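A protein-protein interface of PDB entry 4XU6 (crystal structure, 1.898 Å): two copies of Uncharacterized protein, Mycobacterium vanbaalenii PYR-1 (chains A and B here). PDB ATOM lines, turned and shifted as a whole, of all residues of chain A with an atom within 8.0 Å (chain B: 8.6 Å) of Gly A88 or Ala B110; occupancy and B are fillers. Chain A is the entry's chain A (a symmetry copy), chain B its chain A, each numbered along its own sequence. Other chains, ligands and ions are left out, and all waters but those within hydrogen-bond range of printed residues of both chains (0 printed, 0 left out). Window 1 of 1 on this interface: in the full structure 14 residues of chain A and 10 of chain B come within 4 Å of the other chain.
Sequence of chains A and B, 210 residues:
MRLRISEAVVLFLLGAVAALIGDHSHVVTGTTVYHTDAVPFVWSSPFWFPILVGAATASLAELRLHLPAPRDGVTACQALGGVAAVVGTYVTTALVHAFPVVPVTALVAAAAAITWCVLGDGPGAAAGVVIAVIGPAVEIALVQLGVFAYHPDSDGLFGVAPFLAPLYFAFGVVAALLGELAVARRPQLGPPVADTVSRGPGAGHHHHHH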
ATOM      1  N   ILE A  21       5.859   1.072  16.955  1.00  0.00           N
ATOM      2  CA  ILE A  21       4.712   1.332  16.085  1.00  0.00           C
ATOM      3  C   ILE A  21       4.124   0.014  15.584  1.00  0.00           C
ATOM      4  O   ILE A  21       2.908  -0.193  15.622  1.00  0.00           O
ATOM      5  CB  ILE A  21       5.104   2.225  14.886  1.00  0.00           C
ATOM      6  CG1 ILE A  21       5.459   3.637  15.364  1.00  0.00           C
ATOM      7  CG2 ILE A  21       3.962   2.285  13.849  1.00  0.00           C
ATOM      8  CD1 ILE A  21       6.221   4.472  14.310  1.00  0.00           C
ATOM      9  N   LEU A  80      15.444   5.684   3.701  1.00  0.00           N
ATOM     10  CA  LEU A  80      14.102   6.089   4.120  1.00  0.00           C
ATOM     11  C   LEU A  80      13.055   5.191   3.467  1.00  0.00           C
ATOM     12  O   LEU A  80      12.122   4.731   4.127  1.00  0.00           O
ATOM     13  CB  LEU A  80      13.830   7.555   3.764  1.00  0.00           C
ATOM     14  CG  LEU A  80      12.391   8.050   3.979  1.00  0.00           C
ATOM     15  CD1 LEU A  80      11.922   7.860   5.423  1.00  0.00           C
ATOM     16  CD2 LEU A  80      12.255   9.517   3.564  1.00  0.00           C
ATOM     17  N   GLY A  81      13.225   4.941   2.169  1.00  0.00           N
ATOM     18  CA  GLY A  81      12.322   4.072   1.438  1.00  0.00           C
ATOM     19  C   GLY A  81      12.303   2.668   2.015  1.00  0.00           C
ATOM     20  O   GLY A  81      11.255   2.043   2.088  1.00  0.00           O
ATOM     21  N   GLY A  82      13.465   2.172   2.429  1.00  0.00           N
ATOM     22  CA  GLY A  82      13.552   0.842   3.000  1.00  0.00           C
ATOM     23  C   GLY A  82      12.893   0.772   4.366  1.00  0.00           C
ATOM     24  O   GLY A  82      12.202  -0.196   4.688  1.00  0.00           O
ATOM     25  N   VAL A  83      13.115   1.789   5.188  1.00  0.00           N
ATOM     26  CA  VAL A  83      12.459   1.818   6.496  1.00  0.00           C
ATOM     27  C   VAL A  83      10.933   1.883   6.329  1.00  0.00           C
ATOM     28  O   VAL A  83      10.181   1.204   7.030  1.00  0.00           O
ATOM     29  CB  VAL A  83      12.979   2.973   7.374  1.00  0.00           C
ATOM     30  CG1 VAL A  83      12.096   3.145   8.607  1.00  0.00           C
ATOM     31  CG2 VAL A  83      14.423   2.694   7.800  1.00  0.00           C
ATOM     32  N   ALA A  84      10.485   2.695   5.379  1.00  0.00           N
ATOM     33  CA  ALA A  84       9.054   2.805   5.094  1.00  0.00           C
ATOM     34  C   ALA A  84       8.478   1.465   4.616  1.00  0.00           C
ATOM     35  O   ALA A  84       7.369   1.091   4.986  1.00  0.00           O
ATOM     36  CB  ALA A  84       8.806   3.907   4.067  1.00  0.00           C
ATOM     37  N   ALA A  85       9.235   0.735   3.802  1.00  0.00           N
ATOM     38  CA  ALA A  85       8.760  -0.552   3.285  1.00  0.00           C
ATOM     39  C   ALA A  85       8.595  -1.561   4.418  1.00  0.00           C
ATOM     40  O   ALA A  85       7.614  -2.301   4.464  1.00  0.00           O
ATOM     41  CB  ALA A  85       9.715  -1.098   2.218  1.00  0.00           C
ATOM     42  N   VAL A  86       9.563  -1.592   5.331  1.00  0.00           N
ATOM     43  CA  VAL A  86       9.510  -2.530   6.460  1.00  0.00           C
ATOM     44  C   VAL A  86       8.385  -2.158   7.432  1.00  0.00           C
ATOM     45  O   VAL A  86       7.612  -3.010   7.864  1.00  0.00           O
ATOM     46  CB  VAL A  86      10.870  -2.604   7.202  1.00  0.00           C
ATOM     47  CG1 VAL A  86      10.737  -3.462   8.473  1.00  0.00           C
ATOM     48  CG2 VAL A  86      11.926  -3.208   6.283  1.00  0.00           C
ATOM     49  N   VAL A  87       8.272  -0.877   7.751  1.00  0.00           N
ATOM     50  CA  VAL A  87       7.183  -0.444   8.620  1.00  0.00           C
ATOM     51  C   VAL A  87       5.811  -0.662   7.971  1.00  0.00           C
ATOM     52  O   VAL A  87       4.887  -1.123   8.625  1.00  0.00           O
ATOM     53  CB  VAL A  87       7.337   1.017   9.064  1.00  0.00           C
ATOM     54  CG1 VAL A  87       6.104   1.461   9.846  1.00  0.00           C
ATOM     55  CG2 VAL A  87       8.583   1.166   9.933  1.00  0.00           C
ATOM     56  N   GLY A  88       5.679  -0.344   6.686  1.00  0.00           N
ATOM     57  CA  GLY A  88       4.415  -0.569   6.002  1.00  0.00           C
ATOM     58  C   GLY A  88       4.053  -2.040   5.971  1.00  0.00           C
ATOM     59  O   GLY A  88       2.893  -2.405   6.138  1.00  0.00           O
ATOM     60  N   THR A  89       5.050  -2.896   5.772  1.00  0.00           N
ATOM     61  CA  THR A  89       4.805  -4.337   5.734  1.00  0.00           C
ATOM     62  C   THR A  89       4.401  -4.839   7.117  1.00  0.00           C
ATOM     63  O   THR A  89       3.489  -5.647   7.262  1.00  0.00           O
ATOM     64  CB  THR A  89       6.059  -5.091   5.243  1.00  0.00           C
ATOM     65  OG1 THR A  89       6.409  -4.625   3.932  1.00  0.00           O
ATOM     66  CG2 THR A  89       5.801  -6.588   5.178  1.00  0.00           C
ATOM     67  N   TYR A  90       5.101  -4.346   8.132  1.00  0.00           N
ATOM     68  CA  TYR A  90       4.827  -4.692   9.527  1.00  0.00           C
ATOM     69  C   TYR A  90       3.373  -4.348   9.893  1.00  0.00           C
ATOM     70  O   TYR A  90       2.615  -5.211  10.381  1.00  0.00           O
ATOM     71  CB  TYR A  90       5.816  -3.904  10.397  1.00  0.00           C
ATOM     72  CG  TYR A  90       6.016  -4.361  11.836  1.00  0.00           C
ATOM     73  CD1 TYR A  90       5.081  -5.149  12.498  1.00  0.00           C
ATOM     74  CD2 TYR A  90       7.157  -3.973  12.529  1.00  0.00           C
ATOM     75  CE1 TYR A  90       5.291  -5.544  13.829  1.00  0.00           C
ATOM     76  CE2 TYR A  90       7.371  -4.363  13.839  1.00  0.00           C
ATOM     77  CZ  TYR A  90       6.444  -5.137  14.478  1.00  0.00           C
ATOM     78  OH  TYR A  90       6.682  -5.500  15.787  1.00  0.00           O
ATOM     79  N   VAL A  91       2.958  -3.105   9.649  1.00  0.00           N
ATOM     80  CA  VAL A  91       1.587  -2.726  10.013  1.00  0.00           C
ATOM     81  C   VAL A  91       0.545  -3.439   9.153  1.00  0.00           C
ATOM     82  O   VAL A  91      -0.563  -3.699   9.614  1.00  0.00           O
ATOM     83  CB  VAL A  91       1.351  -1.187  10.022  1.00  0.00           C
ATOM     84  CG1 VAL A  91       2.264  -0.515  11.054  1.00  0.00           C
ATOM     85  CG2 VAL A  91       1.551  -0.577   8.634  1.00  0.00           C
ATOM     86  N   THR A  92       0.901  -3.776   7.916  1.00  0.00           N
ATOM     87  CA  THR A  92      -0.020  -4.532   7.065  1.00  0.00           C
ATOM     88  C   THR A  92      -0.313  -5.903   7.671  1.00  0.00           C
ATOM     89  O   THR A  92      -1.445  -6.388   7.603  1.00  0.00           O
ATOM     90  CB  THR A  92       0.526  -4.703   5.623  1.00  0.00           C
ATOM     91  OG1 THR A  92       0.629  -3.420   4.993  1.00  0.00           O
ATOM     92  CG2 THR A  92      -0.405  -5.595   4.785  1.00  0.00           C
ATOM     93  N   THR A  93       0.698  -6.529   8.269  1.00  0.00           N
ATOM     94  CA  THR A  93       0.468  -7.836   8.883  1.00  0.00           C
ATOM     95  C   THR A  93      -0.545  -7.731  10.012  1.00  0.00           C
ATOM     96  O   THR A  93      -1.303  -8.653  10.242  1.00  0.00           O
ATOM     97  CB  THR A  93       1.755  -8.523   9.395  1.00  0.00           C
ATOM     98  OG1 THR A  93       2.346  -7.750  10.445  1.00  0.00           O
ATOM     99  CG2 THR A  93       2.755  -8.714   8.257  1.00  0.00           C
ATOM    100  N   ALA A  94      -0.568  -6.594  10.697  1.00  0.00           N
ATOM    101  CA  ALA A  94      -1.572  -6.373  11.737  1.00  0.00           C
ATOM    102  C   ALA A  94      -2.974  -6.294  11.122  1.00  0.00           C
ATOM    103  O   ALA A  94      -3.948  -6.826  11.669  1.00  0.00           O
ATOM    104  CB  ALA A  94      -1.249  -5.099  12.510  1.00  0.00           C
ATOM    105  N   LEU A  95      -3.077  -5.637   9.973  1.00  0.00           N
ATOM    106  CA  LEU A  95      -4.375  -5.483   9.313  1.00  0.00           C
ATOM    107  C   LEU A  95      -4.916  -6.792   8.744  1.00  0.00           C
ATOM    108  O   LEU A  95      -6.122  -6.996   8.715  1.00  0.00           O
ATOM    109  CB  LEU A  95      -4.289  -4.447   8.190  1.00  0.00           C
ATOM    110  CG  LEU A  95      -3.826  -3.046   8.592  1.00  0.00           C
ATOM    111  CD1 LEU A  95      -3.772  -2.118   7.378  1.00  0.00           C
ATOM    112  CD2 LEU A  95      -4.721  -2.471   9.663  1.00  0.00           C
ATOM    113  N   ALA A 111       6.334  -8.573  -0.624  1.00  0.00           N
ATOM    114  CA  ALA A 111       6.825  -7.268  -0.190  1.00  0.00           C
ATOM    115  C   ALA A 111       8.308  -7.345   0.143  1.00  0.00           C
ATOM    116  O   ALA A 111       9.079  -6.452  -0.206  1.00  0.00           O
ATOM    117  CB  ALA A 111       6.027  -6.774   1.020  1.00  0.00           C
ATOM    118  N   LEU A 167       9.096 -11.090   7.037  1.00  0.00           N
ATOM    119  CA  LEU A 167       9.140  -9.775   7.684  1.00  0.00           C
ATOM    120  C   LEU A 167      10.532  -9.501   8.251  1.00  0.00           C
ATOM    121  O   LEU A 167      11.102  -8.443   8.007  1.00  0.00           O
ATOM    122  CB  LEU A 167       8.059  -9.632   8.769  1.00  0.00           C
ATOM    123  CG  LEU A 167       8.040  -8.329   9.586  1.00  0.00           C
ATOM    124  CD1 LEU A 167       7.869  -7.118   8.682  1.00  0.00           C
ATOM    125  CD2 LEU A 167       6.930  -8.382  10.667  1.00  0.00           C
ATOM    126  N   THR B  89      -3.261   4.537  -3.073  1.00  0.00           N
ATOM    127  CA  THR B  89      -3.223   4.855  -1.645  1.00  0.00           C
ATOM    128  C   THR B  89      -4.583   5.371  -1.185  1.00  0.00           C
ATOM    129  O   THR B  89      -5.077   5.007  -0.122  1.00  0.00           O
ATOM    130  CB  THR B  89      -2.130   5.904  -1.348  1.00  0.00           C
ATOM    131  OG1 THR B  89      -0.857   5.392  -1.764  1.00  0.00           O
ATOM    132  CG2 THR B  89      -2.071   6.219   0.136  1.00  0.00           C
ATOM    133  N   PRO B 103      -2.024   1.736  12.912  1.00  0.00           N
ATOM    134  CA  PRO B 103      -1.553   1.025  11.718  1.00  0.00           C
ATOM    135  C   PRO B 103      -2.081   1.621  10.412  1.00  0.00           C
ATOM    136  O   PRO B 103      -1.328   1.645   9.435  1.00  0.00           O
ATOM    137  CB  PRO B 103      -2.080  -0.405  11.913  1.00  0.00           C
ATOM    138  CG  PRO B 103      -3.146  -0.307  12.991  1.00  0.00           C
ATOM    139  CD  PRO B 103      -2.716   0.836  13.858  1.00  0.00           C
ATOM    140  N   VAL B 104      -3.326   2.094  10.383  1.00  0.00           N
ATOM    141  CA  VAL B 104      -3.865   2.724   9.165  1.00  0.00           C
ATOM    142  C   VAL B 104      -3.044   3.949   8.758  1.00  0.00           C
ATOM    143  O   VAL B 104      -2.633   4.089   7.605  1.00  0.00           O
ATOM    144  CB  VAL B 104      -5.355   3.126   9.343  1.00  0.00           C
ATOM    145  CG1 VAL B 104      -5.820   4.010   8.194  1.00  0.00           C
ATOM    146  CG2 VAL B 104      -6.236   1.880   9.463  1.00  0.00           C
ATOM    147  N   THR B 105      -2.803   4.837   9.713  1.00  0.00           N
ATOM    148  CA  THR B 105      -2.052   6.051   9.422  1.00  0.00           C
ATOM    149  C   THR B 105      -0.596   5.748   9.045  1.00  0.00           C
ATOM    150  O   THR B 105      -0.027   6.386   8.149  1.00  0.00           O
ATOM    151  CB  THR B 105      -2.119   7.033  10.606  1.00  0.00           C
ATOM    152  OG1 THR B 105      -3.484   7.143  11.045  1.00  0.00           O
ATOM    153  CG2 THR B 105      -1.601   8.398  10.191  1.00  0.00           C
ATOM    154  N   ALA B 106       0.005   4.771   9.720  1.00  0.00           N
ATOM    155  CA  ALA B 106       1.388   4.388   9.409  1.00  0.00           C
ATOM    156  C   ALA B 106       1.494   3.822   7.993  1.00  0.00           C
ATOM    157  O   ALA B 106       2.475   4.075   7.278  1.00  0.00           O
ATOM    158  CB  ALA B 106       1.898   3.370  10.429  1.00  0.00           C
ATOM    159  N   LEU B 107       0.483   3.058   7.581  1.00  0.00           N
ATOM    160  CA  LEU B 107       0.509   2.456   6.245  1.00  0.00           C
ATOM    161  C   LEU B 107       0.500   3.548   5.168  1.00  0.00           C
ATOM    162  O   LEU B 107       1.289   3.507   4.230  1.00  0.00           O
ATOM    163  CB  LEU B 107      -0.670   1.497   6.052  1.00  0.00           C
ATOM    164  CG  LEU B 107      -0.795   0.885   4.652  1.00  0.00           C
ATOM    165  CD1 LEU B 107       0.450   0.073   4.298  1.00  0.00           C
ATOM    166  CD2 LEU B 107      -2.058   0.017   4.548  1.00  0.00           C
ATOM    167  N   VAL B 108      -0.387   4.527   5.321  1.00  0.00           N
ATOM    168  CA  VAL B 108      -0.477   5.635   4.377  1.00  0.00           C
ATOM    169  C   VAL B 108       0.802   6.478   4.389  1.00  0.00           C
ATOM    170  O   VAL B 108       1.302   6.876   3.335  1.00  0.00           O
ATOM    171  CB  VAL B 108      -1.720   6.512   4.662  1.00  0.00           C
ATOM    172  CG1 VAL B 108      -1.828   7.653   3.637  1.00  0.00           C
ATOM    173  CG2 VAL B 108      -2.972   5.641   4.632  1.00  0.00           C
ATOM    174  N   ALA B 109       1.343   6.735   5.575  1.00  0.00           N
ATOM    175  CA  ALA B 109       2.611   7.461   5.670  1.00  0.00           C
ATOM    176  C   ALA B 109       3.756   6.718   4.978  1.00  0.00           C
ATOM    177  O   ALA B 109       4.621   7.338   4.365  1.00  0.00           O
ATOM    178  CB  ALA B 109       2.965   7.765   7.129  1.00  0.00           C
ATOM    179  N   ALA B 110       3.777   5.395   5.087  1.00  0.00           N
ATOM    180  CA  ALA B 110       4.809   4.605   4.409  1.00  0.00           C
ATOM    181  C   ALA B 110       4.658   4.720   2.898  1.00  0.00           C
ATOM    182  O   ALA B 110       5.634   4.878   2.183  1.00  0.00           O
ATOM    183  CB  ALA B 110       4.749   3.133   4.847  1.00  0.00           C
ATOM    184  N   ALA B 111       3.425   4.633   2.412  1.00  0.00           N
ATOM    185  CA  ALA B 111       3.169   4.750   0.980  1.00  0.00           C
ATOM    186  C   ALA B 111       3.594   6.122   0.477  1.00  0.00           C
ATOM    187  O   ALA B 111       4.192   6.243  -0.591  1.00  0.00           O
ATOM    188  CB  ALA B 111       1.689   4.501   0.680  1.00  0.00           C
ATOM    189  N   ALA B 112       3.302   7.156   1.259  1.00  0.00           N
ATOM    190  CA  ALA B 112       3.670   8.518   0.886  1.00  0.00           C
ATOM    191  C   ALA B 112       5.188   8.729   0.884  1.00  0.00           C
ATOM    192  O   ALA B 112       5.728   9.398   0.003  1.00  0.00           O
ATOM    193  CB  ALA B 112       2.995   9.526   1.826  1.00  0.00           C
ATOM    194  N   ALA B 113       5.871   8.173   1.880  1.00  0.00           N
ATOM    195  CA  ALA B 113       7.328   8.285   1.946  1.00  0.00           C
ATOM    196  C   ALA B 113       7.978   7.582   0.761  1.00  0.00           C
ATOM    197  O   ALA B 113       8.929   8.098   0.164  1.00  0.00           O
ATOM    198  CB  ALA B 113       7.858   7.712   3.257  1.00  0.00           C
ATOM    199  N   ILE B 114       7.477   6.397   0.423  1.00  0.00           N
ATOM    200  CA  ILE B 114       8.043   5.653  -0.700  1.00  0.00           C
ATOM    201  C   ILE B 114       7.808   6.398  -2.016  1.00  0.00           C
ATOM    202  O   ILE B 114       8.710   6.501  -2.854  1.00  0.00           O
ATOM    203  CB  ILE B 114       7.497   4.220  -0.763  1.00  0.00           C
ATOM    204  CG1 ILE B 114       8.099   3.382   0.378  1.00  0.00           C
ATOM    205  CG2 ILE B 114       7.820   3.571  -2.112  1.00  0.00           C
ATOM    206  CD1 ILE B 114       7.331   2.099   0.687  1.00  0.00           C
ATOM    207  N   THR B 115       6.602   6.932  -2.183  1.00  0.00           N
ATOM    208  CA  THR B 115       6.276   7.740  -3.364  1.00  0.00           C
ATOM    209  C   THR B 115       7.261   8.898  -3.524  1.00  0.00           C
ATOM    210  O   THR B 115       7.811   9.115  -4.606  1.00  0.00           O
ATOM    211  CB  THR B 115       4.823   8.279  -3.281  1.00  0.00           C
ATOM    212  OG1 THR B 115       3.931   7.174  -3.155  1.00  0.00           O
ATOM    213  CG2 THR B 115       4.450   9.070  -4.541  1.00  0.00           C
ATOM    214  N   TRP B 116       7.503   9.627  -2.439  1.00  0.00           N
ATOM    215  CA  TRP B 116       8.443  10.736  -2.490  1.00  0.00           C
ATOM    216  C   TRP B 116       9.885  10.272  -2.750  1.00  0.00           C
ATOM    217  O   TRP B 116      10.608  10.890  -3.540  1.00  0.00           O
ATOM    218  CB  TRP B 116       8.387  11.587  -1.215  1.00  0.00           C
ATOM    219  CG  TRP B 116       9.360  12.720  -1.309  1.00  0.00           C
ATOM    220  CD1 TRP B 116       9.236  13.857  -2.063  1.00  0.00           C
ATOM    221  CD2 TRP B 116      10.641  12.796  -0.676  1.00  0.00           C
ATOM    222  NE1 TRP B 116      10.367  14.640  -1.927  1.00  0.00           N
ATOM    223  CE2 TRP B 116      11.241  14.011  -1.077  1.00  0.00           C
ATOM    224  CE3 TRP B 116      11.343  11.953   0.192  1.00  0.00           C
ATOM    225  CZ2 TRP B 116      12.508  14.405  -0.629  1.00  0.00           C
ATOM    226  CZ3 TRP B 116      12.595  12.349   0.642  1.00  0.00           C
ATOM    227  CH2 TRP B 116      13.166  13.559   0.228  1.00  0.00           C
ATOM    228  N   CYS B 117      10.311   9.198  -2.088  1.00  0.00           N
ATOM    229  CA  CYS B 117      11.678   8.695  -2.309  1.00  0.00           C
ATOM    230  C   CYS B 117      11.920   8.314  -3.767  1.00  0.00           C
ATOM    231  O   CYS B 117      12.995   8.568  -4.316  1.00  0.00           O
ATOM    232  CB  CYS B 117      11.971   7.494  -1.413  1.00  0.00           C
ATOM    233  SG  CYS B 117      12.204   7.937   0.319  1.00  0.00           S
ATOM    234  N   PRO B 166      -0.650  12.315   5.341  1.00  0.00           N
ATOM    235  CA  PRO B 166       0.250  11.749   4.324  1.00  0.00           C
ATOM    236  C   PRO B 166      -0.417  11.551   2.957  1.00  0.00           C
ATOM    237  O   PRO B 166       0.287  11.541   1.949  1.00  0.00           O
ATOM    238  CB  PRO B 166       0.664  10.394   4.925  1.00  0.00           C
ATOM    239  CG  PRO B 166      -0.398  10.059   5.931  1.00  0.00           C
ATOM    240  CD  PRO B 166      -0.840  11.396   6.481  1.00  0.00           C
ATOM    241  N   LEU B 167      -1.740  11.396   2.907  1.00  0.00           N
ATOM    242  CA  LEU B 167      -2.395  11.253   1.603  1.00  0.00           C
ATOM    243  C   LEU B 167      -2.249  12.533   0.782  1.00  0.00           C
ATOM    244  O   LEU B 167      -1.852  12.483  -0.377  1.00  0.00           O
ATOM    245  CB  LEU B 167      -3.873  10.848   1.744  1.00  0.00           C
ATOM    246  CG  LEU B 167      -4.706  10.738   0.456  1.00  0.00           C
ATOM    247  CD1 LEU B 167      -4.100   9.727  -0.503  1.00  0.00           C
ATOM    248  CD2 LEU B 167      -6.178  10.382   0.790  1.00  0.00           C
ATOM    249  N   ALA B 170       1.448  13.071  -0.423  1.00  0.00           N
ATOM    250  CA  ALA B 170       1.762  12.313  -1.633  1.00  0.00           C
ATOM    251  C   ALA B 170       1.128  12.956  -2.862  1.00  0.00           C
ATOM    252  O   ALA B 170       1.747  13.029  -3.910  1.00  0.00           O
ATOM    253  CB  ALA B 170       1.307  10.845  -1.492  1.00  0.00           C
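SG of Cys B117 lies within hydrogen-bond range of N of Gly A81.
The backbone carbonyl oxygen (O) of Ala B113 lies within hydrogen-bond range of the side-chain sulfur (SG) of Cys B117, 3.3 Å away. O of Ala A85 sits at hydrogen-bond distance from OG1 of Thr A89, 2.7 Å away. The backbone carbonyl oxygen of Gly A88 lies within hydrogen-bond range of the side-chain hydroxyl of Thr A92 (2.7 Å).
3 positions are printed for both chains. Of the 13 pairs that touch across the chains among the printed residues, none has its exchanged pair printed and touching as well.
Of the printed residues of chain B, Leu A80 touches Cys B117 (3.6 Å). Gly A82 touches none of the printed residues of chain B. Of the printed residues of chain B, Ala A84 touches Ala B110 (3.3 Å) and Ile B114 (3.8 Å). Of chain B, only Leu B107 and Ala B110 come within 4 Å of Gly A88. Of the printed residues of chain B, Thr A92 touches Leu B107. Of the printed residues of chain A, Ala B106 touches Val A91. Of the printed residues of chain A, Leu B107 touches Gly A88, Val A91, Thr A92 and Leu A95. No residue of chain A comes within 4 Å of Ala B109. Of the printed residues of chain A, Ala B110 touches Ala A84 and Gly A88. No residue of chain A comes within 4 Å of Ala B111. The nearest residue of chain B that does not touch Gly A88 is Ala B106 (5.2 Å). The nearest printed residue of chain A that does not touch Pro B103 is Leu A95 (4.04 Å).
Gly A81 touches Ile B114 (O to CG1, 3.8 Å). Ala A84 touches Ala B110. Ala A84 touches Ile B114. Ile B114 touches Ala A85 (CD1 to N, 3.9 Å). CD1 of Leu B107 touches O of Gly A88 (3.9 Å). Gly A88 touches Ala B110 (CA to CB, 3.9 Å). CG2 of Val A91 touches O of Pro B103, at 3.7 Å. CG1 of Val A91 touches CB of Ala B106, 3.95 Å away. Leu B107 touches Val A91. Leu A95 touches Leu B107.
Of the 19 printed residues of chain B, 6 touch a printed residue of chain A. Of the 19 printed residues of chain A, 8 touch a printed residue of chain B. Hydrophobic or aromatic side chains of chain A that line the printed part of chain B: Leu A80, Ala A84, Val A91 and Leu A95. Among the printed residues, 13 pairs touch across the chains.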
